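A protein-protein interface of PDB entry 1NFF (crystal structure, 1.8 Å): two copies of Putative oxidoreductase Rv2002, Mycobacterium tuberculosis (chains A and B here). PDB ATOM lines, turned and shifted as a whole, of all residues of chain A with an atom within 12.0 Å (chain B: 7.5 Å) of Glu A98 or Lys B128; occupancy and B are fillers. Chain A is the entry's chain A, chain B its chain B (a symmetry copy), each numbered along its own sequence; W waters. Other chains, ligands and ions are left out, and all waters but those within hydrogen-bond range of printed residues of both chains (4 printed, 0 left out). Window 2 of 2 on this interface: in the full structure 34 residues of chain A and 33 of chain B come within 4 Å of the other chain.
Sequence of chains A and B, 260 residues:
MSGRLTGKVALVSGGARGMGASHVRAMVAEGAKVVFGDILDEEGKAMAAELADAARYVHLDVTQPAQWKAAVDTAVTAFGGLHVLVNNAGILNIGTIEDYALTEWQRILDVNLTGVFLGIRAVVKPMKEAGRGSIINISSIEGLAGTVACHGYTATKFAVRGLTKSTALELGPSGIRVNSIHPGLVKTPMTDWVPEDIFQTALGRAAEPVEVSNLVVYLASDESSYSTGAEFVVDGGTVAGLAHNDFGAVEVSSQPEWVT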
ATOM      1  N   ILE A  94      -9.473  24.254 -16.222  1.00  0.00           N
ATOM      2  CA  ILE A  94      -8.728  25.070 -17.167  1.00  0.00           C
ATOM      3  C   ILE A  94      -7.431  25.599 -16.587  1.00  0.00           C
ATOM      4  O   ILE A  94      -7.184  25.498 -15.384  1.00  0.00           O
ATOM      5  CB  ILE A  94      -9.571  26.277 -17.628  1.00  0.00           C
ATOM      6  CG1 ILE A  94      -9.901  27.163 -16.424  1.00  0.00           C
ATOM      7  CG2 ILE A  94     -10.853  25.796 -18.295  1.00  0.00           C
ATOM      8  CD1 ILE A  94     -10.657  28.436 -16.775  1.00  0.00           C
ATOM      9  N   GLY A  95      -6.609  26.175 -17.456  1.00  0.00           N
ATOM     10  CA  GLY A  95      -5.343  26.727 -17.022  1.00  0.00           C
ATOM     11  C   GLY A  95      -4.346  26.837 -18.156  1.00  0.00           C
ATOM     12  O   GLY A  95      -4.349  26.030 -19.086  1.00  0.00           O
ATOM     13  N   THR A  96      -3.497  27.854 -18.084  1.00  0.00           N
ATOM     14  CA  THR A  96      -2.474  28.061 -19.094  1.00  0.00           C
ATOM     15  C   THR A  96      -1.429  26.973 -18.913  1.00  0.00           C
ATOM     16  O   THR A  96      -1.397  26.292 -17.886  1.00  0.00           O
ATOM     17  CB  THR A  96      -1.793  29.422 -18.921  1.00  0.00           C
ATOM     18  OG1 THR A  96      -1.221  29.499 -17.608  1.00  0.00           O
ATOM     19  CG2 THR A  96      -2.799  30.548 -19.107  1.00  0.00           C
ATOM     20  N   ILE A  97      -0.569  26.808 -19.910  1.00  0.00           N
ATOM     21  CA  ILE A  97       0.474  25.800 -19.840  1.00  0.00           C
ATOM     22  C   ILE A  97       1.297  25.926 -18.555  1.00  0.00           C
ATOM     23  O   ILE A  97       1.638  24.920 -17.930  1.00  0.00           O
ATOM     24  CB  ILE A  97       1.409  25.903 -21.069  1.00  0.00           C
ATOM     25  CG1 ILE A  97       0.635  25.512 -22.331  1.00  0.00           C
ATOM     26  CG2 ILE A  97       2.624  24.994 -20.895  1.00  0.00           C
ATOM     27  CD1 ILE A  97       1.396  25.742 -23.618  1.00  0.00           C
ATOM     28  N   GLU A  98       1.594  27.158 -18.153  1.00  0.00           N
ATOM     29  CA  GLU A  98       2.396  27.394 -16.952  1.00  0.00           C
ATOM     30  C   GLU A  98       1.679  27.167 -15.626  1.00  0.00           C
ATOM     31  O   GLU A  98       2.228  26.543 -14.714  1.00  0.00           O
ATOM     32  CB  GLU A  98       2.960  28.823 -16.950  1.00  0.00           C
ATOM     33  CG  GLU A  98       4.000  29.105 -18.026  1.00  0.00           C
ATOM     34  CD  GLU A  98       3.403  29.692 -19.291  1.00  0.00           C
ATOM     35  OE1 GLU A  98       2.162  29.669 -19.441  1.00  0.00           O
ATOM     36  OE2 GLU A  98       4.183  30.176 -20.139  1.00  0.00           O
ATOM     37  N   ASP A  99       0.455  27.675 -15.529  1.00  0.00           N
ATOM     38  CA  ASP A  99      -0.335  27.593 -14.305  1.00  0.00           C
ATOM     39  C   ASP A  99      -1.137  26.314 -14.076  1.00  0.00           C
ATOM     40  O   ASP A  99      -1.437  25.968 -12.934  1.00  0.00           O
ATOM     41  CB  ASP A  99      -1.285  28.792 -14.247  1.00  0.00           C
ATOM     42  CG  ASP A  99      -0.551  30.122 -14.295  1.00  0.00           C
ATOM     43  OD1 ASP A  99      -1.213  31.154 -14.533  1.00  0.00           O
ATOM     44  OD2 ASP A  99       0.683  30.138 -14.088  1.00  0.00           O
ATOM     45  N   TYR A 100      -1.488  25.619 -15.153  1.00  0.00           N
ATOM     46  CA  TYR A 100      -2.273  24.390 -15.057  1.00  0.00           C
ATOM     47  C   TYR A 100      -1.558  23.348 -14.190  1.00  0.00           C
ATOM     48  O   TYR A 100      -0.434  22.945 -14.486  1.00  0.00           O
ATOM     49  CB  TYR A 100      -2.524  23.852 -16.470  1.00  0.00           C
ATOM     50  CG  TYR A 100      -3.564  22.757 -16.584  1.00  0.00           C
ATOM     51  CD1 TYR A 100      -4.844  22.914 -16.045  1.00  0.00           C
ATOM     52  CD2 TYR A 100      -3.288  21.590 -17.288  1.00  0.00           C
ATOM     53  CE1 TYR A 100      -5.823  21.931 -16.211  1.00  0.00           C
ATOM     54  CE2 TYR A 100      -4.257  20.601 -17.462  1.00  0.00           C
ATOM     55  CZ  TYR A 100      -5.521  20.779 -16.924  1.00  0.00           C
ATOM     56  OH  TYR A 100      -6.472  19.802 -17.113  1.00  0.00           O
ATOM     57  N   ALA A 101      -2.218  22.919 -13.118  1.00  0.00           N
ATOM     58  CA  ALA A 101      -1.637  21.941 -12.203  1.00  0.00           C
ATOM     59  C   ALA A 101      -1.611  20.530 -12.773  1.00  0.00           C
ATOM     60  O   ALA A 101      -2.579  20.072 -13.386  1.00  0.00           O
ATOM     61  CB  ALA A 101      -2.397  21.947 -10.880  1.00  0.00           C
ATOM     62  N   LEU A 102      -0.500  19.834 -12.558  1.00  0.00           N
ATOM     63  CA  LEU A 102      -0.367  18.469 -13.043  1.00  0.00           C
ATOM     64  C   LEU A 102      -1.442  17.560 -12.456  1.00  0.00           C
ATOM     65  O   LEU A 102      -1.878  16.615 -13.107  1.00  0.00           O
ATOM     66  CB  LEU A 102       1.023  17.917 -12.717  1.00  0.00           C
ATOM     67  CG  LEU A 102       2.165  18.555 -13.517  1.00  0.00           C
ATOM     68  CD1 LEU A 102       3.451  17.786 -13.261  1.00  0.00           C
ATOM     69  CD2 LEU A 102       1.829  18.536 -15.009  1.00  0.00           C
ATOM     70  N   THR A 103      -1.869  17.838 -11.228  1.00  0.00           N
ATOM     71  CA  THR A 103      -2.911  17.019 -10.607  1.00  0.00           C
ATOM     72  C   THR A 103      -4.219  17.176 -11.383  1.00  0.00           C
ATOM     73  O   THR A 103      -4.999  16.229 -11.504  1.00  0.00           O
ATOM     74  CB  THR A 103      -3.141  17.410  -9.128  1.00  0.00           C
ATOM     75  OG1 THR A 103      -3.319  18.827  -9.021  1.00  0.00           O
ATOM     76  CG2 THR A 103      -1.956  16.985  -8.277  1.00  0.00           C
ATOM     77  N   GLU A 104      -4.455  18.374 -11.909  1.00  0.00           N
ATOM     78  CA  GLU A 104      -5.667  18.628 -12.681  1.00  0.00           C
ATOM     79  C   GLU A 104      -5.600  17.885 -14.010  1.00  0.00           C
ATOM     80  O   GLU A 104      -6.598  17.333 -14.470  1.00  0.00           O
ATOM     81  CB  GLU A 104      -5.844  20.128 -12.919  1.00  0.00           C
ATOM     82  CG  GLU A 104      -6.269  20.902 -11.681  1.00  0.00           C
ATOM     83  CD  GLU A 104      -7.593  20.419 -11.117  1.00  0.00           C
ATOM     84  OE1 GLU A 104      -7.637  19.300 -10.560  1.00  0.00           O
ATOM     85  OE2 GLU A 104      -8.597  21.156 -11.235  1.00  0.00           O
ATOM     86  N   TRP A 105      -4.419  17.874 -14.622  1.00  0.00           N
ATOM     87  CA  TRP A 105      -4.222  17.168 -15.882  1.00  0.00           C
ATOM     88  C   TRP A 105      -4.496  15.682 -15.657  1.00  0.00           C
ATOM     89  O   TRP A 105      -5.243  15.058 -16.408  1.00  0.00           O
ATOM     90  CB  TRP A 105      -2.787  17.380 -16.382  1.00  0.00           C
ATOM     91  CG  TRP A 105      -2.357  16.446 -17.483  1.00  0.00           C
ATOM     92  CD1 TRP A 105      -1.690  15.256 -17.339  1.00  0.00           C
ATOM     93  CD2 TRP A 105      -2.540  16.634 -18.894  1.00  0.00           C
ATOM     94  NE1 TRP A 105      -1.445  14.699 -18.571  1.00  0.00           N
ATOM     95  CE2 TRP A 105      -1.956  15.521 -19.543  1.00  0.00           C
ATOM     96  CE3 TRP A 105      -3.137  17.635 -19.673  1.00  0.00           C
ATOM     97  CZ2 TRP A 105      -1.951  15.380 -20.939  1.00  0.00           C
ATOM     98  CZ3 TRP A 105      -3.132  17.498 -21.061  1.00  0.00           C
ATOM     99  CH2 TRP A 105      -2.540  16.376 -21.678  1.00  0.00           C
ATOM    100  N   THR A 147      -8.548  24.973 -27.794  1.00  0.00           N
ATOM    101  CA  THR A 147      -9.001  26.126 -27.028  1.00  0.00           C
ATOM    102  C   THR A 147      -7.889  26.549 -26.074  1.00  0.00           C
ATOM    103  O   THR A 147      -7.302  25.716 -25.387  1.00  0.00           O
ATOM    104  CB  THR A 147     -10.265  25.792 -26.206  1.00  0.00           C
ATOM    105  OG1 THR A 147     -11.318  25.385 -27.089  1.00  0.00           O
ATOM    106  CG2 THR A 147     -10.720  27.009 -25.409  1.00  0.00           C
ATOM    107  N   VAL A 148      -7.600  27.845 -26.040  1.00  0.00           N
ATOM    108  CA  VAL A 148      -6.561  28.366 -25.158  1.00  0.00           C
ATOM    109  C   VAL A 148      -6.832  28.005 -23.692  1.00  0.00           C
ATOM    110  O   VAL A 148      -7.977  28.057 -23.227  1.00  0.00           O
ATOM    111  CB  VAL A 148      -6.455  29.907 -25.282  1.00  0.00           C
ATOM    112  CG1 VAL A 148      -5.443  30.444 -24.281  1.00  0.00           C
ATOM    113  CG2 VAL A 148      -6.045  30.289 -26.700  1.00  0.00           C
ATOM    114  N   ALA A 149      -5.775  27.627 -22.977  1.00  0.00           N
ATOM    115  CA  ALA A 149      -5.868  27.280 -21.556  1.00  0.00           C
ATOM    116  C   ALA A 149      -6.887  26.188 -21.253  1.00  0.00           C
ATOM    117  O   ALA A 149      -7.509  26.182 -20.189  1.00  0.00           O
ATOM    118  CB  ALA A 149      -6.199  28.527 -20.749  1.00  0.00           C
ATOM    119  N   CYS A 150      -7.037  25.251 -22.182  1.00  0.00           N
ATOM    120  CA  CYS A 150      -7.993  24.161 -22.032  1.00  0.00           C
ATOM    121  C   CYS A 150      -7.355  22.880 -22.571  1.00  0.00           C
ATOM    122  O   CYS A 150      -7.960  22.144 -23.345  1.00  0.00           O
ATOM    123  CB  CYS A 150      -9.250  24.507 -22.833  1.00  0.00           C
ATOM    124  SG  CYS A 150     -10.666  23.463 -22.519  1.00  0.00           S
ATOM    125  N   HIS A 151      -6.131  22.614 -22.127  1.00  0.00           N
ATOM    126  CA  HIS A 151      -5.355  21.470 -22.598  1.00  0.00           C
ATOM    127  C   HIS A 151      -5.804  20.084 -22.156  1.00  0.00           C
ATOM    128  O   HIS A 151      -5.876  19.167 -22.977  1.00  0.00           O
ATOM    129  CB  HIS A 151      -3.895  21.719 -22.238  1.00  0.00           C
ATOM    130  CG  HIS A 151      -3.452  23.107 -22.576  1.00  0.00           C
ATOM    131  ND1 HIS A 151      -3.483  23.598 -23.864  1.00  0.00           N
ATOM    132  CD2 HIS A 151      -3.073  24.140 -21.787  1.00  0.00           C
ATOM    133  CE1 HIS A 151      -3.146  24.875 -23.854  1.00  0.00           C
ATOM    134  NE2 HIS A 151      -2.894  25.230 -22.606  1.00  0.00           N
ATOM    135  N   GLY A 152      -6.098  19.922 -20.871  1.00  0.00           N
ATOM    136  CA  GLY A 152      -6.551  18.629 -20.395  1.00  0.00           C
ATOM    137  C   GLY A 152      -7.894  18.277 -21.012  1.00  0.00           C
ATOM    138  O   GLY A 152      -8.120  17.145 -21.444  1.00  0.00           O
ATOM    139  N   LEU B  82      17.006  27.239 -26.952  1.00  0.00           N
ATOM    140  CA  LEU B  82      16.171  26.115 -27.364  1.00  0.00           C
ATOM    141  C   LEU B  82      15.062  26.677 -28.238  1.00  0.00           C
ATOM    142  O   LEU B  82      14.209  27.428 -27.763  1.00  0.00           O
ATOM    143  CB  LEU B  82      15.572  25.403 -26.151  1.00  0.00           C
ATOM    144  CG  LEU B  82      14.764  24.145 -26.491  1.00  0.00           C
ATOM    145  CD1 LEU B  82      15.642  23.158 -27.243  1.00  0.00           C
ATOM    146  CD2 LEU B  82      14.224  23.512 -25.216  1.00  0.00           C
ATOM    147  N   PHE B 117       2.786  16.388 -23.193  1.00  0.00           N
ATOM    148  CA  PHE B 117       2.380  17.596 -22.489  1.00  0.00           C
ATOM    149  C   PHE B 117       3.519  18.104 -21.612  1.00  0.00           C
ATOM    150  O   PHE B 117       3.786  19.303 -21.566  1.00  0.00           O
ATOM    151  CB  PHE B 117       1.144  17.322 -21.629  1.00  0.00           C
ATOM    152  CG  PHE B 117       0.658  18.525 -20.869  1.00  0.00           C
ATOM    153  CD1 PHE B 117       0.329  19.702 -21.536  1.00  0.00           C
ATOM    154  CD2 PHE B 117       0.522  18.478 -19.486  1.00  0.00           C
ATOM    155  CE1 PHE B 117      -0.130  20.818 -20.833  1.00  0.00           C
ATOM    156  CE2 PHE B 117       0.063  19.588 -18.773  1.00  0.00           C
ATOM    157  CZ  PHE B 117      -0.263  20.759 -19.448  1.00  0.00           C
ATOM    158  N   ARG B 121       5.360  21.867 -21.618  1.00  0.00           N
ATOM    159  CA  ARG B 121       5.483  22.681 -20.408  1.00  0.00           C
ATOM    160  C   ARG B 121       6.924  23.099 -20.149  1.00  0.00           C
ATOM    161  O   ARG B 121       7.191  24.236 -19.762  1.00  0.00           O
ATOM    162  CB  ARG B 121       5.005  21.912 -19.168  1.00  0.00           C
ATOM    163  CG  ARG B 121       3.536  21.555 -19.133  1.00  0.00           C
ATOM    164  CD  ARG B 121       3.216  20.701 -17.898  1.00  0.00           C
ATOM    165  NE  ARG B 121       3.273  21.444 -16.636  1.00  0.00           N
ATOM    166  CZ  ARG B 121       4.216  21.297 -15.705  1.00  0.00           C
ATOM    167  NH1 ARG B 121       5.210  20.434 -15.877  1.00  0.00           N
ATOM    168  NH2 ARG B 121       4.151  21.998 -14.582  1.00  0.00           N
ATOM    169  N   VAL B 123       9.594  23.334 -22.335  1.00  0.00           N
ATOM    170  CA  VAL B 123      10.275  24.171 -23.323  1.00  0.00           C
ATOM    171  C   VAL B 123       9.755  25.593 -23.508  1.00  0.00           C
ATOM    172  O   VAL B 123      10.462  26.437 -24.067  1.00  0.00           O
ATOM    173  CB  VAL B 123      10.284  23.505 -24.727  1.00  0.00           C
ATOM    174  CG1 VAL B 123      10.911  22.119 -24.653  1.00  0.00           C
ATOM    175  CG2 VAL B 123       8.862  23.435 -25.284  1.00  0.00           C
ATOM    176  N   VAL B 124       8.544  25.876 -23.041  1.00  0.00           N
ATOM    177  CA  VAL B 124       7.980  27.207 -23.239  1.00  0.00           C
ATOM    178  C   VAL B 124       8.746  28.385 -22.640  1.00  0.00           C
ATOM    179  O   VAL B 124       8.797  29.450 -23.248  1.00  0.00           O
ATOM    180  CB  VAL B 124       6.500  27.282 -22.769  1.00  0.00           C
ATOM    181  CG1 VAL B 124       5.621  26.419 -23.680  1.00  0.00           C
ATOM    182  CG2 VAL B 124       6.379  26.833 -21.327  1.00  0.00           C
ATOM    183  N   LYS B 125       9.356  28.214 -21.470  1.00  0.00           N
ATOM    184  CA  LYS B 125      10.081  29.335 -20.872  1.00  0.00           C
ATOM    185  C   LYS B 125      11.176  29.891 -21.792  1.00  0.00           C
ATOM    186  O   LYS B 125      11.127  31.061 -22.178  1.00  0.00           O
ATOM    187  CB  LYS B 125      10.682  28.950 -19.515  1.00  0.00           C
ATOM    188  CG  LYS B 125      11.368  30.123 -18.818  1.00  0.00           C
ATOM    189  CD  LYS B 125      12.047  29.706 -17.523  1.00  0.00           C
ATOM    190  CE  LYS B 125      12.823  30.870 -16.920  1.00  0.00           C
ATOM    191  NZ  LYS B 125      13.530  30.496 -15.664  1.00  0.00           N
ATOM    192  N   PRO B 126      12.175  29.069 -22.162  1.00  0.00           N
ATOM    193  CA  PRO B 126      13.216  29.613 -23.043  1.00  0.00           C
ATOM    194  C   PRO B 126      12.696  30.061 -24.412  1.00  0.00           C
ATOM    195  O   PRO B 126      13.180  31.044 -24.972  1.00  0.00           O
ATOM    196  CB  PRO B 126      14.231  28.473 -23.138  1.00  0.00           C
ATOM    197  CG  PRO B 126      13.398  27.239 -22.896  1.00  0.00           C
ATOM    198  CD  PRO B 126      12.479  27.677 -21.782  1.00  0.00           C
ATOM    199  N   MET B 127      11.712  29.344 -24.951  1.00  0.00           N
ATOM    200  CA  MET B 127      11.153  29.712 -26.248  1.00  0.00           C
ATOM    201  C   MET B 127      10.491  31.086 -26.195  1.00  0.00           C
ATOM    202  O   MET B 127      10.645  31.890 -27.114  1.00  0.00           O
ATOM    203  CB  MET B 127      10.138  28.669 -26.719  1.00  0.00           C
ATOM    204  CG  MET B 127      10.755  27.337 -27.121  1.00  0.00           C
ATOM    205  SD  MET B 127       9.566  26.298 -27.995  1.00  0.00           S
ATOM    206  CE  MET B 127      10.578  24.850 -28.393  1.00  0.00           C
ATOM    207  N   LYS B 128       9.757  31.356 -25.120  1.00  0.00           N
ATOM    208  CA  LYS B 128       9.098  32.646 -24.975  1.00  0.00           C
ATOM    209  C   LYS B 128      10.117  33.769 -24.802  1.00  0.00           C
ATOM    210  O   LYS B 128       9.908  34.885 -25.278  1.00  0.00           O
ATOM    211  CB  LYS B 128       8.130  32.628 -23.790  1.00  0.00           C
ATOM    212  CG  LYS B 128       6.854  31.838 -24.056  1.00  0.00           C
ATOM    213  CD  LYS B 128       5.824  32.063 -22.958  1.00  0.00           C
ATOM    214  CE  LYS B 128       4.508  31.376 -23.292  1.00  0.00           C
ATOM    215  NZ  LYS B 128       3.471  31.635 -22.253  1.00  0.00           N
ATOM    216  N   GLU B 129      11.223  33.475 -24.126  1.00  0.00           N
ATOM    217  CA  GLU B 129      12.258  34.485 -23.919  1.00  0.00           C
ATOM    218  C   GLU B 129      12.902  34.814 -25.260  1.00  0.00           C
ATOM    219  O   GLU B 129      13.256  35.964 -25.527  1.00  0.00           O
ATOM    220  CB  GLU B 129      13.326  33.975 -22.948  1.00  0.00           C
ATOM    221  CG  GLU B 129      12.784  33.543 -21.600  1.00  0.00           C
ATOM    222  CD  GLU B 129      13.873  33.034 -20.678  1.00  0.00           C
ATOM    223  OE1 GLU B 129      14.805  32.360 -21.168  1.00  0.00           O
ATOM    224  OE2 GLU B 129      13.788  33.294 -19.461  1.00  0.00           O
ATOM    225  N   ALA B 130      13.042  33.796 -26.103  1.00  0.00           N
ATOM    226  CA  ALA B 130      13.638  33.968 -27.420  1.00  0.00           C
ATOM    227  C   ALA B 130      12.657  34.641 -28.372  1.00  0.00           C
ATOM    228  O   ALA B 130      13.063  35.253 -29.356  1.00  0.00           O
ATOM    229  CB  ALA B 130      14.066  32.616 -27.980  1.00  0.00           C
ATOM    230  N   GLY B 131      11.366  34.522 -28.074  1.00  0.00           N
ATOM    231  CA  GLY B 131      10.352  35.128 -28.918  1.00  0.00           C
ATOM    232  C   GLY B 131      10.052  34.320 -30.168  1.00  0.00           C
ATOM    233  O   GLY B 131       9.355  34.787 -31.066  1.00  0.00           O
ATOM    234  N   ARG B 132      10.587  33.103 -30.235  1.00  0.00           N
ATOM    235  CA  ARG B 132      10.361  32.245 -31.386  1.00  0.00           C
ATOM    236  C   ARG B 132      10.625  30.785 -31.055  1.00  0.00           C
ATOM    237  O   ARG B 132      11.509  30.464 -30.257  1.00  0.00           O
ATOM    238  CB  ARG B 132      11.232  32.687 -32.572  1.00  0.00           C
ATOM    239  CG  ARG B 132      12.725  32.856 -32.282  1.00  0.00           C
ATOM    240  CD  ARG B 132      13.451  33.382 -33.527  1.00  0.00           C
ATOM    241  NE  ARG B 132      14.827  33.818 -33.278  1.00  0.00           N
ATOM    242  CZ  ARG B 132      15.871  33.006 -33.136  1.00  0.00           C
ATOM    243  NH1 ARG B 132      15.716  31.689 -33.218  1.00  0.00           N
ATOM    244  NH2 ARG B 132      17.079  33.512 -32.917  1.00  0.00           N
ATOM    245  N   GLY B 133       9.840  29.902 -31.662  1.00  0.00           N
ATOM    246  CA  GLY B 133      10.006  28.487 -31.411  1.00  0.00           C
ATOM    247  C   GLY B 133       9.055  27.646 -32.235  1.00  0.00           C
ATOM    248  O   GLY B 133       8.063  28.141 -32.772  1.00  0.00           O
ATOM    249  N   GLU B 170      -2.669  28.959 -27.743  1.00  0.00           N
ATOM    250  CA  GLU B 170      -2.152  29.694 -26.594  1.00  0.00           C
ATOM    251  C   GLU B 170      -0.750  30.271 -26.791  1.00  0.00           C
ATOM    252  O   GLU B 170      -0.462  31.388 -26.344  1.00  0.00           O
ATOM    253  CB  GLU B 170      -2.157  28.790 -25.359  1.00  0.00           C
ATOM    254  CG  GLU B 170      -1.716  29.495 -24.081  1.00  0.00           C
ATOM    255  CD  GLU B 170      -1.822  28.603 -22.860  1.00  0.00           C
ATOM    256  OE1 GLU B 170      -2.906  28.019 -22.644  1.00  0.00           O
ATOM    257  OE2 GLU B 170      -0.825  28.490 -22.112  1.00  0.00           O
ATOM    258  N   LEU B 171       0.114  29.520 -27.468  1.00  0.00           N
ATOM    259  CA  LEU B 171       1.493  29.939 -27.684  1.00  0.00           C
ATOM    260  C   LEU B 171       1.766  30.821 -28.907  1.00  0.00           C
ATOM    261  O   LEU B 171       2.808  31.475 -28.979  1.00  0.00           O
ATOM    262  CB  LEU B 171       2.398  28.703 -27.733  1.00  0.00           C
ATOM    263  CG  LEU B 171       2.450  27.849 -26.458  1.00  0.00           C
ATOM    264  CD1 LEU B 171       3.295  26.600 -26.704  1.00  0.00           C
ATOM    265  CD2 LEU B 171       3.028  28.675 -25.310  1.00  0.00           C
ATOM    266  N   PRO B 173       0.765  33.783 -29.844  1.00  0.00           N
ATOM    267  CA  PRO B 173       1.083  35.181 -29.525  1.00  0.00           C
ATOM    268  C   PRO B 173       2.525  35.392 -29.053  1.00  0.00           C
ATOM    269  O   PRO B 173       3.054  36.504 -29.131  1.00  0.00           O
ATOM    270  CB  PRO B 173       0.062  35.525 -28.445  1.00  0.00           C
ATOM    271  CG  PRO B 173      -1.124  34.688 -28.841  1.00  0.00           C
ATOM    272  CD  PRO B 173      -0.469  33.363 -29.158  1.00  0.00           C
ATOM    273  N   SER B 174       3.154  34.327 -28.558  1.00  0.00           N
ATOM    274  CA  SER B 174       4.533  34.403 -28.075  1.00  0.00           C
ATOM    275  C   SER B 174       5.554  34.034 -29.151  1.00  0.00           C
ATOM    276  O   SER B 174       6.758  33.981 -28.883  1.00  0.00           O
ATOM    277  CB  SER B 174       4.723  33.486 -26.859  1.00  0.00           C
ATOM    278  OG  SER B 174       3.916  33.900 -25.769  1.00  0.00           O
ATOM    279  N   GLY B 175       5.072  33.774 -30.363  1.00  0.00           N
ATOM    280  CA  GLY B 175       5.959  33.424 -31.459  1.00  0.00           C
ATOM    281  C   GLY B 175       6.307  31.947 -31.541  1.00  0.00           C
ATOM    282  O   GLY B 175       7.249  31.565 -32.230  1.00  0.00           O
ATOM    283  N   ILE B 176       5.543  31.114 -30.845  1.00  0.00           N
ATOM    284  CA  ILE B 176       5.791  29.676 -30.839  1.00  0.00           C
ATOM    285  C   ILE B 176       4.724  28.913 -31.609  1.00  0.00           C
ATOM    286  O   ILE B 176       3.537  29.014 -31.299  1.00  0.00           O
ATOM    287  CB  ILE B 176       5.832  29.136 -29.396  1.00  0.00           C
ATOM    288  CG1 ILE B 176       6.950  29.833 -28.618  1.00  0.00           C
ATOM    289  CG2 ILE B 176       6.044  27.627 -29.407  1.00  0.00           C
ATOM    290  CD1 ILE B 176       6.862  29.652 -27.116  1.00  0.00           C
HETATM  291  O   HOH W   1       3.855  24.403 -16.502  1.00  0.00           O
HETATM  292  O   HOH W   2       1.919  23.872 -13.545  1.00  0.00           O
HETATM  293  O   HOH W   3       0.913  22.582 -16.627  1.00  0.00           O
HETATM  294  O   HOH W   4       1.055  30.210 -21.837  1.00  0.00           O
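Glu B170 touches Thr A96.
CA of Arg B121 touches CG2 of Ile A97, 3.7 Å away.
CD1 of Ile A97 touches CG of Leu B171, at 3.7 Å.
Phe B117 touches Tyr A100.
Leu A102 touches Arg B121 (CD2 to NE, 3.6 Å).
Trp A105 touches Phe B117 (CD2 to CD2, 3.6 Å).
Glu B170 touches Val A148.
No position is printed for both chains.
Of the 11 pairs that touch across the chains among the printed residues, none has its exchanged pair printed and touching as well.
Gly A95 touches none of the printed residues of chain B.
Of the printed residues of chain B, Ile A97 touches Arg B121 (3.7 Å), Glu B170 (2.8 Å) and Leu B171 (3.7 Å).
Glu A98 touches just one residue of chain B: Lys B128.
Printed residues of chain B within 4 Å of Tyr A100: Phe B117.
Of the printed residues of chain B, Val A148 touches Glu B170.
Of the printed residues of chain B, Ala A149 touches Glu B170 (2.9 Å).
Printed residues of chain B within 4 Å of His A151: Glu B170.
Gly A152 touches none of the printed residues of chain B.
Of the printed residues of chain A, Arg B121 touches Ile A97 (3.7 Å) and Leu A102 (3.6 Å).
No residue of chain A comes within 4 Å of Val B124.
No residue of chain A comes within 4 Å of Pro B126.
No residue of chain A comes within 4 Å of Met B127.
No residue of chain A comes within 4 Å of Glu B129.
No residue of chain A comes within 4 Å of Ala B130.
No residue of chain A comes within 4 Å of Gly B131.
Printed residues of chain A within 4 Å of Leu B171: Ile A97 (3.7 Å).
No residue of chain A comes within 4 Å of Gly B175.
The nearest residue of chain A that does not touch Lys B128 is Ile A97 (6.2 Å).
The nearest printed residue of chain A that does not touch Phe B117 is His A151 (4.1 Å).
OE2 of Glu A98 is in salt-bridge range of NZ of Lys B128, at 2.7 Å.
N of Ala A149 lies within hydrogen-bond range of OE1 of Glu B170, at 2.9 Å.
The backbone NH of Ile A97 lies within hydrogen-bond range of the side-chain carboxylate of Glu B170, 2.8 Å away.
OE1 of Glu B170 lies within hydrogen-bond range of NE2 of His A151.
Water W3 lies within hydrogen-bond range of O of Tyr A100 (2.6 Å), NE of Arg B121 (2.6 Å) and O of Ile A97 (2.8 Å).
Water W4 lies within hydrogen-bond range of OE2 of Glu B170 (2.6 Å), OE1 of Glu A98 (2.7 Å) and NZ of Lys B128 (2.8 Å).
Water W1 lies within hydrogen-bond range of O of Ile A97, NE of Arg B121 and O of Glu A98.
Water W2 lies within hydrogen-bond range of the backbone carbonyl oxygen (O) of Tyr A100, the backbone carbonyl oxygen (O) of Glu A98 and the guanidinium group (NH2) of Arg B121.
Of the 18 printed residues of chain A, 9 touch a printed residue of chain B.
Hydrophobic or aromatic side chains of chain A within 4 Å of the printed part of chain B: Ile A97, Tyr A100, Leu A102, Trp A105, Val A148, Ala A149 and His A151.
Of the 20 printed residues of chain B, 5 touch a printed residue of chain A.
The backbone carbonyl oxygen of Leu B171 is in hydrogen-bond range of the backbone NH of Ile B176, 3.3 Å away.
OG1 of Thr A96 sits at hydrogen-bond distance from N of Asp A99 (3.2 Å).
N of Gly A95 sits at hydrogen-bond distance from O of Ala A149 (2.9 Å).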
